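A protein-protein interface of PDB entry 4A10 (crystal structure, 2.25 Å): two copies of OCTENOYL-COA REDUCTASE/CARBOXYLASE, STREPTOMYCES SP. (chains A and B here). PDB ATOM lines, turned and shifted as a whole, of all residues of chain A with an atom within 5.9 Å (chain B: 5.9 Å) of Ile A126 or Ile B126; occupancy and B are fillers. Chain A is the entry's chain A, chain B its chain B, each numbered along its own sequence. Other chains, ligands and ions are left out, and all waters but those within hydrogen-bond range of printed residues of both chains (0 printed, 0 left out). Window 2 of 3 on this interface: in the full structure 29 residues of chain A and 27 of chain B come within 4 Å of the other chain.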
ATOM      1  N   ALA A  61     -25.521  23.445 -19.059  1.00  0.00           N
ATOM      2  CA  ALA A  61     -26.381  22.238 -19.015  1.00  0.00           C
ATOM      3  C   ALA A  61     -25.903  21.208 -17.959  1.00  0.00           C
ATOM      4  O   ALA A  61     -24.755  21.266 -17.520  1.00  0.00           O
ATOM      5  CB  ALA A  61     -26.491  21.582 -20.405  1.00  0.00           C
ATOM      6  N   PRO A  62     -26.778  20.253 -17.573  1.00  0.00           N
ATOM      7  CA  PRO A  62     -26.484  19.301 -16.496  1.00  0.00           C
ATOM      8  C   PRO A  62     -25.234  18.444 -16.721  1.00  0.00           C
ATOM      9  O   PRO A  62     -24.584  18.035 -15.758  1.00  0.00           O
ATOM     10  CB  PRO A  62     -27.726  18.391 -16.497  1.00  0.00           C
ATOM     11  CG  PRO A  62     -28.784  19.185 -17.112  1.00  0.00           C
ATOM     12  CD  PRO A  62     -28.118  20.003 -18.147  1.00  0.00           C
ATOM     13  N   ASP A  63     -24.910  18.165 -17.975  1.00  0.00           N
ATOM     14  CA  ASP A  63     -23.801  17.256 -18.293  1.00  0.00           C
ATOM     15  C   ASP A  63     -22.594  18.034 -18.836  1.00  0.00           C
ATOM     16  O   ASP A  63     -21.676  17.457 -19.441  1.00  0.00           O
ATOM     17  CB  ASP A  63     -24.257  16.164 -19.270  1.00  0.00           C
ATOM     18  CG  ASP A  63     -24.776  16.729 -20.606  1.00  0.00           C
ATOM     19  OD1 ASP A  63     -25.241  17.898 -20.657  1.00  0.00           O
ATOM     20  OD2 ASP A  63     -24.725  15.998 -21.637  1.00  0.00           O
ATOM     21  N   TRP A 102     -31.515  21.941 -24.437  1.00  0.00           N
ATOM     22  CA  TRP A 102     -30.257  22.672 -24.189  1.00  0.00           C
ATOM     23  C   TRP A 102     -29.487  23.069 -25.466  1.00  0.00           C
ATOM     24  O   TRP A 102     -28.702  24.018 -25.453  1.00  0.00           O
ATOM     25  CB  TRP A 102     -29.363  21.880 -23.210  1.00  0.00           C
ATOM     26  CG  TRP A 102     -29.961  21.783 -21.806  1.00  0.00           C
ATOM     27  CD1 TRP A 102     -30.692  20.759 -21.312  1.00  0.00           C
ATOM     28  CD2 TRP A 102     -29.879  22.760 -20.750  1.00  0.00           C
ATOM     29  NE1 TRP A 102     -31.068  21.018 -20.020  1.00  0.00           N
ATOM     30  CE2 TRP A 102     -30.587  22.240 -19.647  1.00  0.00           C
ATOM     31  CE3 TRP A 102     -29.266  24.014 -20.626  1.00  0.00           C
ATOM     32  CZ2 TRP A 102     -30.709  22.928 -18.433  1.00  0.00           C
ATOM     33  CZ3 TRP A 102     -29.386  24.704 -19.408  1.00  0.00           C
ATOM     34  CH2 TRP A 102     -30.106  24.152 -18.334  1.00  0.00           C
ATOM     35  N   THR A 124     -19.206  22.727 -12.813  1.00  0.00           N
ATOM     36  CA  THR A 124     -19.722  21.494 -13.397  1.00  0.00           C
ATOM     37  C   THR A 124     -21.241  21.453 -13.257  1.00  0.00           C
ATOM     38  O   THR A 124     -21.773  21.895 -12.246  1.00  0.00           O
ATOM     39  CB  THR A 124     -19.135  20.237 -12.724  1.00  0.00           C
ATOM     40  OG1 THR A 124     -19.685  20.102 -11.418  1.00  0.00           O
ATOM     41  CG2 THR A 124     -17.616  20.321 -12.613  1.00  0.00           C
ATOM     42  N   GLY A 125     -21.932  20.925 -14.266  1.00  0.00           N
ATOM     43  CA  GLY A 125     -23.378  20.733 -14.173  1.00  0.00           C
ATOM     44  C   GLY A 125     -23.663  19.690 -13.104  1.00  0.00           C
ATOM     45  O   GLY A 125     -22.759  18.928 -12.726  1.00  0.00           O
ATOM     46  N   ILE A 126     -24.906  19.644 -12.615  1.00  0.00           N
ATOM     47  CA  ILE A 126     -25.247  18.721 -11.521  1.00  0.00           C
ATOM     48  C   ILE A 126     -25.244  17.239 -11.935  1.00  0.00           C
ATOM     49  O   ILE A 126     -25.360  16.366 -11.079  1.00  0.00           O
ATOM     50  CB  ILE A 126     -26.585  19.068 -10.785  1.00  0.00           C
ATOM     51  CG1 ILE A 126     -27.809  18.650 -11.617  1.00  0.00           C
ATOM     52  CG2 ILE A 126     -26.609  20.544 -10.276  1.00  0.00           C
ATOM     53  CD1 ILE A 126     -28.184  19.579 -12.769  1.00  0.00           C
ATOM     54  N   GLY A 127     -25.114  16.959 -13.232  1.00  0.00           N
ATOM     55  CA  GLY A 127     -24.996  15.569 -13.703  1.00  0.00           C
ATOM     56  C   GLY A 127     -23.579  15.152 -14.058  1.00  0.00           C
ATOM     57  O   GLY A 127     -23.369  14.099 -14.655  1.00  0.00           O
ATOM     58  N   VAL A 128     -22.597  15.971 -13.694  1.00  0.00           N
ATOM     59  CA  VAL A 128     -21.193  15.639 -13.957  1.00  0.00           C
ATOM     60  C   VAL A 128     -20.602  14.834 -12.788  1.00  0.00           C
ATOM     61  O   VAL A 128     -20.747  15.196 -11.617  1.00  0.00           O
ATOM     62  CB  VAL A 128     -20.341  16.913 -14.298  1.00  0.00           C
ATOM     63  CG1 VAL A 128     -18.853  16.588 -14.423  1.00  0.00           C
ATOM     64  CG2 VAL A 128     -20.849  17.559 -15.587  1.00  0.00           C
ATOM     65  N   ALA B  61     -32.110  11.341 -10.541  1.00  0.00           N
ATOM     66  CA  ALA B  61     -30.916  12.027 -11.085  1.00  0.00           C
ATOM     67  C   ALA B  61     -31.177  12.673 -12.463  1.00  0.00           C
ATOM     68  O   ALA B  61     -32.122  12.293 -13.163  1.00  0.00           O
ATOM     69  CB  ALA B  61     -29.721  11.072 -11.145  1.00  0.00           C
ATOM     70  N   PRO B  62     -30.324  13.637 -12.864  1.00  0.00           N
ATOM     71  CA  PRO B  62     -30.601  14.447 -14.051  1.00  0.00           C
ATOM     72  C   PRO B  62     -30.631  13.681 -15.379  1.00  0.00           C
ATOM     73  O   PRO B  62     -31.291  14.119 -16.339  1.00  0.00           O
ATOM     74  CB  PRO B  62     -29.475  15.487 -14.057  1.00  0.00           C
ATOM     75  CG  PRO B  62     -28.470  15.028 -13.090  1.00  0.00           C
ATOM     76  CD  PRO B  62     -29.096  14.060 -12.163  1.00  0.00           C
ATOM     77  N   ASP B  63     -29.937  12.548 -15.420  1.00  0.00           N
ATOM     78  CA  ASP B  63     -29.857  11.714 -16.620  1.00  0.00           C
ATOM     79  C   ASP B  63     -30.764  10.458 -16.480  1.00  0.00           C
ATOM     80  O   ASP B  63     -30.639   9.473 -17.228  1.00  0.00           O
ATOM     81  CB  ASP B  63     -28.392  11.333 -16.848  1.00  0.00           C
ATOM     82  CG  ASP B  63     -27.874  10.316 -15.820  1.00  0.00           C
ATOM     83  OD1 ASP B  63     -28.141  10.454 -14.601  1.00  0.00           O
ATOM     84  OD2 ASP B  63     -27.194   9.346 -16.236  1.00  0.00           O
ATOM     85  N   TRP B 102     -24.900  10.915  -6.949  1.00  0.00           N
ATOM     86  CA  TRP B 102     -26.181  10.234  -7.155  1.00  0.00           C
ATOM     87  C   TRP B 102     -26.151   8.736  -6.840  1.00  0.00           C
ATOM     88  O   TRP B 102     -27.193   8.159  -6.504  1.00  0.00           O
ATOM     89  CB  TRP B 102     -26.705  10.502  -8.578  1.00  0.00           C
ATOM     90  CG  TRP B 102     -27.019  11.976  -8.772  1.00  0.00           C
ATOM     91  CD1 TRP B 102     -26.206  12.921  -9.334  1.00  0.00           C
ATOM     92  CD2 TRP B 102     -28.203  12.665  -8.359  1.00  0.00           C
ATOM     93  NE1 TRP B 102     -26.816  14.146  -9.311  1.00  0.00           N
ATOM     94  CE2 TRP B 102     -28.045  14.020  -8.722  1.00  0.00           C
ATOM     95  CE3 TRP B 102     -29.389  12.268  -7.730  1.00  0.00           C
ATOM     96  CZ2 TRP B 102     -29.032  14.990  -8.474  1.00  0.00           C
ATOM     97  CZ3 TRP B 102     -30.375  13.237  -7.483  1.00  0.00           C
ATOM     98  CH2 TRP B 102     -30.179  14.580  -7.848  1.00  0.00           C
ATOM     99  N   THR B 124     -38.755  12.678 -16.261  1.00  0.00           N
ATOM    100  CA  THR B 124     -37.351  12.666 -16.707  1.00  0.00           C
ATOM    101  C   THR B 124     -36.549  13.719 -15.966  1.00  0.00           C
ATOM    102  O   THR B 124     -37.063  14.797 -15.660  1.00  0.00           O
ATOM    103  CB  THR B 124     -37.186  12.936 -18.224  1.00  0.00           C
ATOM    104  OG1 THR B 124     -37.675  14.255 -18.526  1.00  0.00           O
ATOM    105  CG2 THR B 124     -37.935  11.892 -19.063  1.00  0.00           C
ATOM    106  N   GLY B 125     -35.286  13.407 -15.683  1.00  0.00           N
ATOM    107  CA  GLY B 125     -34.357  14.396 -15.133  1.00  0.00           C
ATOM    108  C   GLY B 125     -34.120  15.481 -16.172  1.00  0.00           C
ATOM    109  O   GLY B 125     -34.342  15.257 -17.361  1.00  0.00           O
ATOM    110  N   ILE B 126     -33.670  16.655 -15.723  1.00  0.00           N
ATOM    111  CA  ILE B 126     -33.508  17.807 -16.614  1.00  0.00           C
ATOM    112  C   ILE B 126     -32.410  17.640 -17.702  1.00  0.00           C
ATOM    113  O   ILE B 126     -32.313  18.460 -18.632  1.00  0.00           O
ATOM    114  CB  ILE B 126     -33.367  19.179 -15.835  1.00  0.00           C
ATOM    115  CG1 ILE B 126     -31.941  19.426 -15.298  1.00  0.00           C
ATOM    116  CG2 ILE B 126     -34.477  19.359 -14.767  1.00  0.00           C
ATOM    117  CD1 ILE B 126     -31.414  18.403 -14.311  1.00  0.00           C
ATOM    118  N   GLY B 127     -31.594  16.596 -17.588  1.00  0.00           N
ATOM    119  CA  GLY B 127     -30.567  16.320 -18.613  1.00  0.00           C
ATOM    120  C   GLY B 127     -30.983  15.284 -19.644  1.00  0.00           C
ATOM    121  O   GLY B 127     -30.216  14.954 -20.539  1.00  0.00           O
ATOM    122  N   VAL B 128     -32.207  14.780 -19.533  1.00  0.00           N
ATOM    123  CA  VAL B 128     -32.706  13.744 -20.452  1.00  0.00           C
ATOM    124  C   VAL B 128     -33.214  14.349 -21.775  1.00  0.00           C
ATOM    125  O   VAL B 128     -34.036  15.246 -21.776  1.00  0.00           O
ATOM    126  CB  VAL B 128     -33.777  12.838 -19.743  1.00  0.00           C
ATOM    127  CG1 VAL B 128     -34.452  11.881 -20.718  1.00  0.00           C
ATOM    128  CG2 VAL B 128     -33.134  12.051 -18.613  1.00  0.00           C
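The indole nitrogen (NE1) of Trp A102 lies within hydrogen-bond range of the backbone carbonyl oxygen (O) of Ile B126.
The backbone carbonyl oxygen (O) of Ile A126 is in hydrogen-bond range of the indole nitrogen (NE1) of Trp B102 (3.2 Å).
Of the 9 printed residues of chain A, 4 touch a printed residue of chain B.
Hydrophobic or aromatic side chains of chain B that line the printed part of chain A: Pro B62, Trp B102 and Ile B126.
Among the printed residues, 7 pairs touch across the chains.
The backbone NH (N) of Gly A127 sits at hydrogen-bond distance from the backbone carbonyl oxygen (O) of Pro A62.
O of Pro B62 is in hydrogen-bond range of N of Gly B127 (2.8 Å).
The backbone NH of Val B128 is in hydrogen-bond range of the backbone carbonyl oxygen of Pro B62.
Pro A62 touches Ile B126, and with the chains exchanged Ile A126 touches Pro B62.
Pro A62 touches Gly B127, and with the chains exchanged Gly A127 touches Pro B62.
Trp A102 touches Ile B126, and with the chains exchanged Ile A126 touches Trp B102.
Ile A126 touches its own counterpart, Ile B126.
Ala A61 touches none of the printed residues of chain B.
Of the printed residues of chain B, Pro A62 touches Ile B126 (3.6 Å) and Gly B127 (3.7 Å).
Of chain B, only Pro B62 (3.9 Å), Trp B102 (3.2 Å) and Ile B126 (3.8 Å) come within 4 Å of Ile A126.
Of the printed residues of chain B, Gly A127 touches Pro B62.
Asp B63 touches none of the printed residues of chain A.
Printed residues of chain A within 4 Å of Trp B102: Ile A126.
Of the printed residues of chain A, Gly B127 touches Pro A62.
The nearest printed residue of chain B that does not touch Ile A126 is Gly B127 (6.6 Å).
The nearest printed residue of chain A that does not touch Ile B126 is Gly A127 (6.6 Å).
The nearest printed residue of chain B that does not touch Gly A127 is Trp B102 (5.0 Å).
Among the printed residues, merely in contact across the chains: Gly A127 with Pro B62 (3.6 Å), Pro A62 with Ile B126 (3.6 Å), Pro A62 with Gly B127 (3.7 Å), Ile A126 with Ile B126 (3.8 Å) and Ile A126 with Pro B62 (3.9 Å).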
